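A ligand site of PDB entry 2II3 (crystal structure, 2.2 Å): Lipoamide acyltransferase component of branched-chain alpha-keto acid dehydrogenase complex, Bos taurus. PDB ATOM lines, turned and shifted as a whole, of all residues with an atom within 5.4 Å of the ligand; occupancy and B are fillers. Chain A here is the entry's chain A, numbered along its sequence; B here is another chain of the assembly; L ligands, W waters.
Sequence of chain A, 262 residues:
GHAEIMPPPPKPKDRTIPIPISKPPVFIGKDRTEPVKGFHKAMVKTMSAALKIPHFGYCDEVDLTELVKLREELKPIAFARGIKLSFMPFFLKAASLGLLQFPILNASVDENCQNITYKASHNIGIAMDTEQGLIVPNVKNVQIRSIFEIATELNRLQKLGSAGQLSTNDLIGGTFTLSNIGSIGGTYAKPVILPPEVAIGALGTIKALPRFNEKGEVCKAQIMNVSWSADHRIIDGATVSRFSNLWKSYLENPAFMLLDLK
O4 of the ligand lies within salt-bridge range of NH2 of Arg 71, 2.4 Å away.
The side-chain hydroxyl (OG) of Ser 179 sits at hydrogen-bond distance from a nitrogen (N7) of the ligand, at 2.7 Å.
The backbone carbonyl oxygen (O) of Gly 204 lies within hydrogen-bond range of a nitrogen (N3) of the ligand (2.7 Å).
O12 of the ligand sits at hydrogen-bond distance from OG of Ser 86.
The backbone carbonyl oxygen of Asn 180 sits close to a nitrogen (N6) of the ligand (3.3 Å).
ND2 of Asn 180 lies within hydrogen-bond range of N4 of the ligand (2.8 Å).
The side-chain carboxylate (OD1) of Asp 129 sits at hydrogen-bond distance from an oxygen (O17) of the ligand (2.8 Å).
The backbone NH of Ile 206 is in hydrogen-bond range of a nitrogen (N1) of the ligand (2.9 Å).
N of Gly 237 of chain B is in hydrogen-bond range of O17 of the ligand (2.9 Å).
S1 of the ligand lies close to NE2 of His 232 of chain B, 3.1 Å away.
The side-chain hydroxyl (OG) of Ser 183 lies within hydrogen-bond range of a nitrogen (N6) of the ligand.
NZ of Lys 75 lies within salt-bridge range of O4 of the ligand, 3.9 Å away.
NE of Arg 71 lies within hydrogen-bond range of O of Leu 85.
O of Ser 179 lies within hydrogen-bond range of N of Leu 203, 2.9 Å away.
The backbone carbonyl oxygen (O) of Asn 180 is in hydrogen-bond range of the side-chain hydroxyl (OG) of Ser 183 (3.1 Å).
N of Gly 237 of chain B sits at hydrogen-bond distance from OD2 of Asp 129 (3.4 Å).
O of Gly 182 lies within hydrogen-bond range of OG1 of Thr 205 (3.3 Å).
The backbone NH of Gly 182 is in hydrogen-bond range of the backbone carbonyl oxygen of Leu 203, 2.8 Å away.
OD1 of Asp 236 of chain B lies close to N of Ala 238 of chain B, at 3.4 Å.
The backbone NH (N) of Ile 181 sits close to the backbone carbonyl oxygen (O) of Leu 203, at 3.2 Å.
Merely in contact with the ligand: Met 88, Phe 87, Ile 126, Leu 134, Ala 127, Gly 182, Thr 205, Asp 236 of chain B, Gln 158, Met 128, Phe 56 of chain B and Ile 181.
Hydrophobic or aromatic side chains within 4 Å of the ligand: Phe 87, Met 88, Ile 126, Met 128, Leu 134, Ile 181, Ile 206, Phe 56 of chain B and His 232 of chain B.
23 residues have an atom within 4 Å of the ligand: Arg 71, Lys 75, Ser 86, Phe 87, Met 88, Ile 126, Ala 127, Met 128, Asp 129, Leu 134, Gln 158, Ser 179, Asn 180, Ile 181, Gly 182, Ser 183, Gly 204, Thr 205, Ile 206, Phe 56 of chain B, His 232 of chain B, Asp 236 of chain B and Gly 237 of chain B.
Water W3 lies within hydrogen-bond range of the side-chain amide oxygen of Gln 158 (2.4 Å), an oxygen (O12) of the ligand (2.8 Å) and the side-chain hydroxyl of Ser 86 (3.3 Å).
Water W4 bridges O of Ser 183 and O6 of the ligand.
Water W1 bridges the backbone NH of Asn 180 (2.8 Å) and the backbone carbonyl oxygen of Ala 127 (2.9 Å).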
ATOM      1  N   ARG A  71     -22.917 -18.924  17.173  1.00  0.00           N
ATOM      2  CA  ARG A  71     -21.555 -18.424  16.944  1.00  0.00           C
ATOM      3  C   ARG A  71     -20.655 -18.607  18.176  1.00  0.00           C
ATOM      4  O   ARG A  71     -19.480 -18.994  18.062  1.00  0.00           O
ATOM      5  CB  ARG A  71     -21.575 -16.977  16.485  1.00  0.00           C
ATOM      6  CG  ARG A  71     -20.210 -16.370  16.446  1.00  0.00           C
ATOM      7  CD  ARG A  71     -20.304 -14.951  15.993  1.00  0.00           C
ATOM      8  NE  ARG A  71     -19.007 -14.319  16.114  1.00  0.00           N
ATOM      9  CZ  ARG A  71     -18.632 -13.561  17.145  1.00  0.00           C
ATOM     10  NH1 ARG A  71     -19.443 -13.337  18.177  1.00  0.00           N
ATOM     11  NH2 ARG A  71     -17.425 -13.039  17.122  1.00  0.00           N
ATOM     12  N   LYS A  75     -17.095 -20.506  18.075  1.00  0.00           N
ATOM     13  CA  LYS A  75     -15.910 -19.645  18.220  1.00  0.00           C
ATOM     14  C   LYS A  75     -14.615 -20.352  18.587  1.00  0.00           C
ATOM     15  O   LYS A  75     -13.610 -20.092  17.924  1.00  0.00           O
ATOM     16  CB  LYS A  75     -16.168 -18.444  19.163  1.00  0.00           C
ATOM     17  CG  LYS A  75     -16.877 -17.255  18.482  1.00  0.00           C
ATOM     18  CD  LYS A  75     -16.569 -15.865  19.156  1.00  0.00           C
ATOM     19  CE  LYS A  75     -17.383 -15.646  20.425  1.00  0.00           C
ATOM     20  NZ  LYS A  75     -17.030 -14.386  21.150  1.00  0.00           N
ATOM     21  N   LYS A  84     -10.678 -16.266  13.002  1.00  0.00           N
ATOM     22  CA  LYS A  84     -11.677 -15.528  13.752  1.00  0.00           C
ATOM     23  C   LYS A  84     -12.980 -15.661  12.973  1.00  0.00           C
ATOM     24  O   LYS A  84     -13.020 -15.428  11.759  1.00  0.00           O
ATOM     25  CB  LYS A  84     -11.321 -14.038  13.847  1.00  0.00           C
ATOM     26  CG  LYS A  84     -10.036 -13.683  14.649  1.00  0.00           C
ATOM     27  CD  LYS A  84      -9.690 -12.194  14.333  1.00  0.00           C
ATOM     28  CE  LYS A  84      -9.278 -11.346  15.590  1.00  0.00           C
ATOM     29  NZ  LYS A  84      -9.649  -9.838  15.495  1.00  0.00           N
ATOM     30  N   LEU A  85     -14.044 -15.993  13.675  1.00  0.00           N
ATOM     31  CA  LEU A  85     -15.364 -16.218  13.062  1.00  0.00           C
ATOM     32  C   LEU A  85     -16.336 -15.176  13.549  1.00  0.00           C
ATOM     33  O   LEU A  85     -16.770 -15.189  14.699  1.00  0.00           O
ATOM     34  CB  LEU A  85     -15.868 -17.638  13.403  1.00  0.00           C
ATOM     35  CG  LEU A  85     -17.326 -18.011  13.112  1.00  0.00           C
ATOM     36  CD1 LEU A  85     -17.585 -18.068  11.592  1.00  0.00           C
ATOM     37  CD2 LEU A  85     -17.729 -19.321  13.836  1.00  0.00           C
ATOM     38  N   SER A  86     -16.677 -14.214  12.691  1.00  0.00           N
ATOM     39  CA  SER A  86     -17.610 -13.188  13.079  1.00  0.00           C
ATOM     40  C   SER A  86     -19.018 -13.643  12.646  1.00  0.00           C
ATOM     41  O   SER A  86     -19.230 -14.827  12.339  1.00  0.00           O
ATOM     42  CB  SER A  86     -17.200 -11.875  12.429  1.00  0.00           C
ATOM     43  OG  SER A  86     -17.414 -11.957  11.026  1.00  0.00           O
ATOM     44  N   PHE A  87     -19.967 -12.708  12.556  1.00  0.00           N
ATOM     45  CA  PHE A  87     -21.244 -13.021  12.001  1.00  0.00           C
ATOM     46  C   PHE A  87     -21.243 -13.003  10.470  1.00  0.00           C
ATOM     47  O   PHE A  87     -22.110 -13.618   9.850  1.00  0.00           O
ATOM     48  CB  PHE A  87     -22.304 -12.050  12.517  1.00  0.00           C
ATOM     49  CG  PHE A  87     -22.562 -12.160  13.998  1.00  0.00           C
ATOM     50  CD1 PHE A  87     -23.512 -13.081  14.487  1.00  0.00           C
ATOM     51  CD2 PHE A  87     -21.864 -11.348  14.916  1.00  0.00           C
ATOM     52  CE1 PHE A  87     -23.762 -13.189  15.871  1.00  0.00           C
ATOM     53  CE2 PHE A  87     -22.095 -11.443  16.272  1.00  0.00           C
ATOM     54  CZ  PHE A  87     -23.057 -12.374  16.777  1.00  0.00           C
ATOM     55  N   MET A  88     -20.269 -12.316   9.854  1.00  0.00           N
ATOM     56  CA  MET A  88     -20.294 -12.103   8.386  1.00  0.00           C
ATOM     57  C   MET A  88     -20.358 -13.396   7.532  1.00  0.00           C
ATOM     58  O   MET A  88     -21.101 -13.435   6.520  1.00  0.00           O
ATOM     59  CB  MET A  88     -19.108 -11.215   7.947  1.00  0.00           C
ATOM     60  CG  MET A  88     -19.333  -9.686   8.182  1.00  0.00           C
ATOM     61  SD  MET A  88     -20.766  -9.104   7.318  1.00  0.00           S
ATOM     62  CE  MET A  88     -20.093  -8.775   5.685  1.00  0.00           C
ATOM     63  N   PRO A  89     -19.532 -14.419   7.873  1.00  0.00           N
ATOM     64  CA  PRO A  89     -19.599 -15.687   7.125  1.00  0.00           C
ATOM     65  C   PRO A  89     -20.973 -16.322   7.117  1.00  0.00           C
ATOM     66  O   PRO A  89     -21.371 -16.909   6.128  1.00  0.00           O
ATOM     67  CB  PRO A  89     -18.619 -16.548   7.870  1.00  0.00           C
ATOM     68  CG  PRO A  89     -17.613 -15.560   8.394  1.00  0.00           C
ATOM     69  CD  PRO A  89     -18.497 -14.496   8.909  1.00  0.00           C
ATOM     70  N   PHE A  91     -23.886 -14.434   7.428  1.00  0.00           N
ATOM     71  CA  PHE A  91     -24.670 -13.548   6.583  1.00  0.00           C
ATOM     72  C   PHE A  91     -24.421 -13.831   5.106  1.00  0.00           C
ATOM     73  O   PHE A  91     -25.331 -13.715   4.297  1.00  0.00           O
ATOM     74  CB  PHE A  91     -24.351 -12.040   6.864  1.00  0.00           C
ATOM     75  CG  PHE A  91     -24.659 -11.589   8.275  1.00  0.00           C
ATOM     76  CD1 PHE A  91     -25.587 -12.300   9.094  1.00  0.00           C
ATOM     77  CD2 PHE A  91     -24.012 -10.478   8.810  1.00  0.00           C
ATOM     78  CE1 PHE A  91     -25.888 -11.866  10.419  1.00  0.00           C
ATOM     79  CE2 PHE A  91     -24.269 -10.064  10.150  1.00  0.00           C
ATOM     80  CZ  PHE A  91     -25.227 -10.750  10.931  1.00  0.00           C
ATOM     81  N   ILE A 126     -17.427  -7.217   0.250  1.00  0.00           N
ATOM     82  CA  ILE A 126     -17.411  -6.772   1.636  1.00  0.00           C
ATOM     83  C   ILE A 126     -17.013  -5.298   1.582  1.00  0.00           C
ATOM     84  O   ILE A 126     -15.866  -5.035   1.373  1.00  0.00           O
ATOM     85  CB  ILE A 126     -16.277  -7.544   2.399  1.00  0.00           C
ATOM     86  CG1 ILE A 126     -16.323  -9.042   2.005  1.00  0.00           C
ATOM     87  CG2 ILE A 126     -16.365  -7.311   3.925  1.00  0.00           C
ATOM     88  CD1 ILE A 126     -17.719  -9.659   2.348  1.00  0.00           C
ATOM     89  N   ALA A 127     -17.950  -4.351   1.735  1.00  0.00           N
ATOM     90  CA  ALA A 127     -17.553  -2.957   1.781  1.00  0.00           C
ATOM     91  C   ALA A 127     -16.705  -2.733   3.043  1.00  0.00           C
ATOM     92  O   ALA A 127     -17.112  -3.120   4.122  1.00  0.00           O
ATOM     93  CB  ALA A 127     -18.779  -2.028   1.752  1.00  0.00           C
ATOM     94  N   MET A 128     -15.483  -2.237   2.868  1.00  0.00           N
ATOM     95  CA  MET A 128     -14.635  -1.824   3.994  1.00  0.00           C
ATOM     96  C   MET A 128     -14.105  -0.425   3.699  1.00  0.00           C
ATOM     97  O   MET A 128     -13.991  -0.008   2.541  1.00  0.00           O
ATOM     98  CB  MET A 128     -13.522  -2.848   4.358  1.00  0.00           C
ATOM     99  CG  MET A 128     -12.942  -3.773   3.294  1.00  0.00           C
ATOM    100  SD  MET A 128     -11.475  -4.790   3.844  1.00  0.00           S
ATOM    101  CE  MET A 128     -12.245  -6.423   4.075  1.00  0.00           C
ATOM    102  N   ASP A 129     -13.893   0.382   4.731  1.00  0.00           N
ATOM    103  CA  ASP A 129     -13.316   1.731   4.472  1.00  0.00           C
ATOM    104  C   ASP A 129     -11.946   1.647   5.079  1.00  0.00           C
ATOM    105  O   ASP A 129     -11.780   1.183   6.200  1.00  0.00           O
ATOM    106  CB  ASP A 129     -14.144   2.909   5.067  1.00  0.00           C
ATOM    107  CG  ASP A 129     -15.497   3.128   4.366  1.00  0.00           C
ATOM    108  OD1 ASP A 129     -15.518   3.282   3.110  1.00  0.00           O
ATOM    109  OD2 ASP A 129     -16.560   3.136   5.046  1.00  0.00           O
ATOM    110  N   LEU A 134     -12.984   3.941   0.337  1.00  0.00           N
ATOM    111  CA  LEU A 134     -13.826   2.789   0.060  1.00  0.00           C
ATOM    112  C   LEU A 134     -13.134   1.712  -0.744  1.00  0.00           C
ATOM    113  O   LEU A 134     -12.739   1.908  -1.902  1.00  0.00           O
ATOM    114  CB  LEU A 134     -15.145   3.176  -0.639  1.00  0.00           C
ATOM    115  CG  LEU A 134     -16.075   1.966  -0.883  1.00  0.00           C
ATOM    116  CD1 LEU A 134     -16.607   1.373   0.461  1.00  0.00           C
ATOM    117  CD2 LEU A 134     -17.193   2.259  -1.913  1.00  0.00           C
ATOM    118  N   LEU A 154     -12.365 -14.320   4.575  1.00  0.00           N
ATOM    119  CA  LEU A 154     -12.621 -13.028   5.163  1.00  0.00           C
ATOM    120  C   LEU A 154     -11.465 -12.512   5.955  1.00  0.00           C
ATOM    121  O   LEU A 154     -11.179 -11.321   5.899  1.00  0.00           O
ATOM    122  CB  LEU A 154     -13.811 -13.041   6.100  1.00  0.00           C
ATOM    123  CG  LEU A 154     -15.168 -13.002   5.440  1.00  0.00           C
ATOM    124  CD1 LEU A 154     -16.256 -12.791   6.487  1.00  0.00           C
ATOM    125  CD2 LEU A 154     -15.202 -11.869   4.400  1.00  0.00           C
ATOM    126  N   GLN A 158      -9.467  -9.073   5.212  1.00  0.00           N
ATOM    127  CA  GLN A 158      -9.191  -8.112   6.314  1.00  0.00           C
ATOM    128  C   GLN A 158      -7.681  -7.904   6.557  1.00  0.00           C
ATOM    129  O   GLN A 158      -7.212  -6.790   6.747  1.00  0.00           O
ATOM    130  CB  GLN A 158      -9.845  -8.523   7.648  1.00  0.00           C
ATOM    131  CG  GLN A 158     -11.366  -8.590   7.706  1.00  0.00           C
ATOM    132  CD  GLN A 158     -11.863  -8.996   9.125  1.00  0.00           C
ATOM    133  OE1 GLN A 158     -12.520 -10.036   9.295  1.00  0.00           O
ATOM    134  NE2 GLN A 158     -11.509  -8.197  10.135  1.00  0.00           N
ATOM    135  N   SER A 179     -22.660  -4.603   3.252  1.00  0.00           N
ATOM    136  CA  SER A 179     -21.940  -3.598   4.016  1.00  0.00           C
ATOM    137  C   SER A 179     -22.308  -3.738   5.504  1.00  0.00           C
ATOM    138  O   SER A 179     -23.441  -3.469   5.918  1.00  0.00           O
ATOM    139  CB  SER A 179     -22.345  -2.206   3.502  1.00  0.00           C
ATOM    140  OG  SER A 179     -21.568  -1.224   4.151  1.00  0.00           O
ATOM    141  N   ASN A 180     -21.377  -4.223   6.299  1.00  0.00           N
ATOM    142  CA  ASN A 180     -21.616  -4.369   7.723  1.00  0.00           C
ATOM    143  C   ASN A 180     -21.402  -3.009   8.374  1.00  0.00           C
ATOM    144  O   ASN A 180     -20.388  -2.802   9.008  1.00  0.00           O
ATOM    145  CB  ASN A 180     -20.700  -5.461   8.287  1.00  0.00           C
ATOM    146  CG  ASN A 180     -21.014  -5.797   9.747  1.00  0.00           C
ATOM    147  OD1 ASN A 180     -22.068  -5.440  10.267  1.00  0.00           O
ATOM    148  ND2 ASN A 180     -20.048  -6.466  10.425  1.00  0.00           N
ATOM    149  N   ILE A 181     -22.326  -2.059   8.183  1.00  0.00           N
ATOM    150  CA  ILE A 181     -22.155  -0.746   8.837  1.00  0.00           C
ATOM    151  C   ILE A 181     -22.118  -0.966  10.388  1.00  0.00           C
ATOM    152  O   ILE A 181     -21.430  -0.246  11.115  1.00  0.00           O
ATOM    153  CB  ILE A 181     -23.276   0.312   8.425  1.00  0.00           C
ATOM    154  CG1 ILE A 181     -24.629  -0.182   8.876  1.00  0.00           C
ATOM    155  CG2 ILE A 181     -23.365   0.382   6.917  1.00  0.00           C
ATOM    156  CD1 ILE A 181     -25.776   0.842   9.280  1.00  0.00           C
ATOM    157  N   GLY A 182     -22.877  -1.968  10.870  1.00  0.00           N
ATOM    158  CA  GLY A 182     -22.989  -2.233  12.314  1.00  0.00           C
ATOM    159  C   GLY A 182     -21.734  -2.656  13.040  1.00  0.00           C
ATOM    160  O   GLY A 182     -21.744  -2.717  14.238  1.00  0.00           O
ATOM    161  N   SER A 183     -20.621  -2.930  12.338  1.00  0.00           N
ATOM    162  CA  SER A 183     -19.368  -3.224  13.042  1.00  0.00           C
ATOM    163  C   SER A 183     -18.916  -1.952  13.705  1.00  0.00           C
ATOM    164  O   SER A 183     -18.075  -1.993  14.641  1.00  0.00           O
ATOM    165  CB  SER A 183     -18.264  -3.738  12.097  1.00  0.00           C
ATOM    166  OG  SER A 183     -18.044  -2.823  11.022  1.00  0.00           O
ATOM    167  N   ILE A 184     -19.442  -0.822  13.197  1.00  0.00           N
ATOM    168  CA  ILE A 184     -19.233   0.505  13.793  1.00  0.00           C
ATOM    169  C   ILE A 184     -20.477   1.075  14.532  1.00  0.00           C
ATOM    170  O   ILE A 184     -20.365   1.523  15.664  1.00  0.00           O
ATOM    171  CB  ILE A 184     -18.771   1.575  12.749  1.00  0.00           C
ATOM    172  CG1 ILE A 184     -17.481   1.134  12.052  1.00  0.00           C
ATOM    173  CG2 ILE A 184     -18.579   2.952  13.492  1.00  0.00           C
ATOM    174  CD1 ILE A 184     -16.940   2.085  10.962  1.00  0.00           C
ATOM    175  N   LEU A 203     -26.064  -3.990   7.054  1.00  0.00           N
ATOM    176  CA  LEU A 203     -26.380  -4.619   8.331  1.00  0.00           C
ATOM    177  C   LEU A 203     -26.080  -3.685   9.459  1.00  0.00           C
ATOM    178  O   LEU A 203     -25.008  -3.102   9.500  1.00  0.00           O
ATOM    179  CB  LEU A 203     -25.578  -5.900   8.510  1.00  0.00           C
ATOM    180  CG  LEU A 203     -25.592  -6.596   7.151  1.00  0.00           C
ATOM    181  CD1 LEU A 203     -24.318  -7.373   6.913  1.00  0.00           C
ATOM    182  CD2 LEU A 203     -26.865  -7.405   7.004  1.00  0.00           C
ATOM    183  N   GLY A 204     -27.056  -3.518  10.362  1.00  0.00           N
ATOM    184  CA  GLY A 204     -26.906  -2.605  11.465  1.00  0.00           C
ATOM    185  C   GLY A 204     -26.281  -3.270  12.646  1.00  0.00           C
ATOM    186  O   GLY A 204     -25.895  -4.422  12.578  1.00  0.00           O
ATOM    187  N   THR A 205     -26.233  -2.550  13.766  1.00  0.00           N
ATOM    188  CA  THR A 205     -25.688  -3.061  15.018  1.00  0.00           C
ATOM    189  C   THR A 205     -26.684  -4.078  15.592  1.00  0.00           C
ATOM    190  O   THR A 205     -27.905  -3.802  15.676  1.00  0.00           O
ATOM    191  CB  THR A 205     -25.405  -1.924  16.046  1.00  0.00           C
ATOM    192  OG1 THR A 205     -24.335  -1.099  15.559  1.00  0.00           O
ATOM    193  CG2 THR A 205     -24.956  -2.525  17.411  1.00  0.00           C
ATOM    194  N   ILE A 206     -26.168  -5.282  15.923  1.00  0.00           N
ATOM    195  CA  ILE A 206     -26.929  -6.251  16.729  1.00  0.00           C
ATOM    196  C   ILE A 206     -27.073  -5.731  18.150  1.00  0.00           C
ATOM    197  O   ILE A 206     -26.092  -5.444  18.808  1.00  0.00           O
ATOM    198  CB  ILE A 206     -26.248  -7.635  16.736  1.00  0.00           C
ATOM    199  CG1 ILE A 206     -25.858  -8.085  15.328  1.00  0.00           C
ATOM    200  CG2 ILE A 206     -27.123  -8.636  17.513  1.00  0.00           C
ATOM    201  CD1 ILE A 206     -24.900  -9.296  15.315  1.00  0.00           C
ATOM    202  N   MET A 224     -31.188  -7.387  14.765  1.00  0.00           N
ATOM    203  CA  MET A 224     -30.354  -6.700  13.820  1.00  0.00           C
ATOM    204  C   MET A 224     -31.225  -6.146  12.728  1.00  0.00           C
ATOM    205  O   MET A 224     -32.124  -6.802  12.224  1.00  0.00           O
ATOM    206  CB  MET A 224     -29.306  -7.634  13.201  1.00  0.00           C
ATOM    207  CG  MET A 224     -28.155  -6.885  12.543  1.00  0.00           C
ATOM    208  SD  MET A 224     -27.043  -7.860  11.527  1.00  0.00           S
ATOM    209  CE  MET A 224     -28.122  -8.598  10.286  1.00  0.00           C
ATOM    210  N   PHE B  56     -26.051   8.812   0.458  1.00  0.00           N
ATOM    211  CA  PHE B  56     -25.920   7.590   1.291  1.00  0.00           C
ATOM    212  C   PHE B  56     -26.722   7.838   2.557  1.00  0.00           C
ATOM    213  O   PHE B  56     -26.547   8.893   3.170  1.00  0.00           O
ATOM    214  CB  PHE B  56     -24.421   7.393   1.705  1.00  0.00           C
ATOM    215  CG  PHE B  56     -24.195   6.314   2.736  1.00  0.00           C
ATOM    216  CD1 PHE B  56     -24.421   4.970   2.417  1.00  0.00           C
ATOM    217  CD2 PHE B  56     -23.707   6.628   3.992  1.00  0.00           C
ATOM    218  CE1 PHE B  56     -24.217   3.926   3.382  1.00  0.00           C
ATOM    219  CE2 PHE B  56     -23.498   5.629   4.954  1.00  0.00           C
ATOM    220  CZ  PHE B  56     -23.754   4.262   4.653  1.00  0.00           C
ATOM    221  N   HIS B 232     -22.060  10.712  -1.002  1.00  0.00           N
ATOM    222  CA  HIS B 232     -21.157   9.530  -1.027  1.00  0.00           C
ATOM    223  C   HIS B 232     -19.942   9.565  -1.994  1.00  0.00           C
ATOM    224  O   HIS B 232     -19.073   8.667  -1.929  1.00  0.00           O
ATOM    225  CB  HIS B 232     -21.926   8.215  -1.175  1.00  0.00           C
ATOM    226  CG  HIS B 232     -21.270   7.081  -0.472  1.00  0.00           C
ATOM    227  ND1 HIS B 232     -19.903   7.030  -0.245  1.00  0.00           N
ATOM    228  CD2 HIS B 232     -21.761   5.928   0.036  1.00  0.00           C
ATOM    229  CE1 HIS B 232     -19.594   5.905   0.374  1.00  0.00           C
ATOM    230  NE2 HIS B 232     -20.704   5.230   0.578  1.00  0.00           N
ATOM    231  N   ASP B 236     -17.462   8.597   3.136  1.00  0.00           N
ATOM    232  CA  ASP B 236     -17.743   7.155   3.195  1.00  0.00           C
ATOM    233  C   ASP B 236     -18.556   6.800   4.440  1.00  0.00           C
ATOM    234  O   ASP B 236     -18.872   7.676   5.302  1.00  0.00           O
ATOM    235  CB  ASP B 236     -16.456   6.323   3.048  1.00  0.00           C
ATOM    236  CG  ASP B 236     -15.448   6.581   4.154  1.00  0.00           C
ATOM    237  OD1 ASP B 236     -15.835   6.950   5.270  1.00  0.00           O
ATOM    238  OD2 ASP B 236     -14.255   6.392   3.918  1.00  0.00           O
ATOM    239  N   GLY B 237     -18.928   5.528   4.533  1.00  0.00           N
ATOM    240  CA  GLY B 237     -19.859   5.058   5.553  1.00  0.00           C
ATOM    241  C   GLY B 237     -19.304   5.165   6.942  1.00  0.00           C
ATOM    242  O   GLY B 237     -20.025   5.467   7.904  1.00  0.00           O
ATOM    243  N   ALA B 238     -17.995   4.979   7.038  1.00  0.00           N
ATOM    244  CA  ALA B 238     -17.304   4.933   8.323  1.00  0.00           C
ATOM    245  C   ALA B 238     -17.260   6.296   8.915  1.00  0.00           C
ATOM    246  O   ALA B 238     -17.457   6.447  10.111  1.00  0.00           O
ATOM    247  CB  ALA B 238     -15.872   4.360   8.167  1.00  0.00           C
HETATM  248  N1  LIG L   1     -23.445  -5.818  15.244  1.00  0.00           N
HETATM  249  C1  LIG L   1     -22.816  -6.074  16.421  1.00  0.00           C
HETATM  250  N2  LIG L   1     -21.558  -6.563  16.500  1.00  0.00           N
HETATM  251  C2  LIG L   1     -20.833  -6.779  15.371  1.00  0.00           C
HETATM  252  C3  LIG L   1     -21.442  -6.522  14.052  1.00  0.00           C
HETATM  253  C4  LIG L   1     -22.853  -6.004  14.028  1.00  0.00           C
HETATM  254  N3  LIG L   1     -23.489  -5.726  12.834  1.00  0.00           N
HETATM  255  N4  LIG L   1     -20.520  -6.821  13.117  1.00  0.00           N
HETATM  256  C5  LIG L   1     -19.414  -7.240  13.792  1.00  0.00           C
HETATM  257  N5  LIG L   1     -19.596  -7.199  15.126  1.00  0.00           N
HETATM  258  C6  LIG L   1     -18.605  -7.615  16.156  1.00  0.00           C
HETATM  259  C7  LIG L   1     -18.171  -9.052  15.906  1.00  0.00           C
HETATM  260  O1  LIG L   1     -19.094  -9.849  16.596  1.00  0.00           O
HETATM  261  C8  LIG L   1     -16.835  -9.147  16.608  1.00  0.00           C
HETATM  262  O2  LIG L   1     -17.107  -9.338  18.000  1.00  0.00           O
HETATM  263  P1  LIG L   1     -16.189 -10.146  19.062  1.00  0.00           P
HETATM  264  O3  LIG L   1     -14.841  -9.442  18.880  1.00  0.00           O
HETATM  265  O4  LIG L   1     -16.162 -11.580  18.575  1.00  0.00           O
HETATM  266  O5  LIG L   1     -16.921 -10.007  20.347  1.00  0.00           O
HETATM  267  C9  LIG L   1     -16.276  -7.736  16.463  1.00  0.00           C
HETATM  268  O6  LIG L   1     -17.374  -6.861  16.151  1.00  0.00           O
HETATM  269  C10 LIG L   1     -15.247  -7.718  15.346  1.00  0.00           C
HETATM  270  O7  LIG L   1     -15.829  -7.834  14.042  1.00  0.00           O
HETATM  271  P2  LIG L   1     -14.847  -7.427  12.807  1.00  0.00           P
HETATM  272  O8  LIG L   1     -13.451  -7.923  13.170  1.00  0.00           O
HETATM  273  O9  LIG L   1     -15.028  -5.985  12.372  1.00  0.00           O
HETATM  274  O10 LIG L   1     -15.229  -8.424  11.594  1.00  0.00           O
HETATM  275  P3  LIG L   1     -16.591  -8.525  10.726  1.00  0.00           P
HETATM  276  O11 LIG L   1     -17.767  -8.440  11.678  1.00  0.00           O
HETATM  277  O12 LIG L   1     -16.336  -9.740   9.803  1.00  0.00           O
HETATM  278  O13 LIG L   1     -16.638  -7.279   9.695  1.00  0.00           O
HETATM  279  C11 LIG L   1     -15.717  -5.917   7.910  1.00  0.00           C
HETATM  280  C12 LIG L   1     -15.586  -7.194   8.729  1.00  0.00           C
HETATM  281  C13 LIG L   1     -16.968  -6.068   7.049  1.00  0.00           C
HETATM  282  C14 LIG L   1     -14.480  -5.798   7.021  1.00  0.00           C
HETATM  283  C15 LIG L   1     -15.811  -4.714   8.882  1.00  0.00           C
HETATM  284  O14 LIG L   1     -14.724  -4.637   9.860  1.00  0.00           O
HETATM  285  C16 LIG L   1     -15.953  -3.384   8.137  1.00  0.00           C
HETATM  286  O15 LIG L   1     -14.967  -2.783   7.680  1.00  0.00           O
HETATM  287  N6  LIG L   1     -17.227  -2.969   8.039  1.00  0.00           N
HETATM  288  C17 LIG L   1     -17.600  -1.594   7.756  1.00  0.00           C
HETATM  289  C18 LIG L   1     -18.738  -1.512   6.733  1.00  0.00           C
HETATM  290  C19 LIG L   1     -18.678  -0.116   6.185  1.00  0.00           C
HETATM  291  O16 LIG L   1     -17.736   0.624   6.514  1.00  0.00           O
HETATM  292  N7  LIG L   1     -19.684   0.253   5.366  1.00  0.00           N
HETATM  293  C20 LIG L   1     -19.983   1.682   5.135  1.00  0.00           C
HETATM  294  C21 LIG L   1     -20.827   2.017   3.897  1.00  0.00           C
HETATM  295  S1  LIG L   1     -20.064   2.995   2.579  1.00  0.00           S
HETATM  296  O17 LIG L   1     -18.327   3.307   2.719  1.00  0.00           O
HETATM  297  O   HOH W   1     -18.928  -5.002   5.291  1.00  0.00           O
HETATM  298  O   HOH W   2     -23.312   0.929   2.824  1.00  0.00           O
HETATM  299  O   HOH W   3     -14.278 -11.573   9.915  1.00  0.00           O
HETATM  300  O   HOH W   4     -17.084  -4.055  16.190  1.00  0.00           O
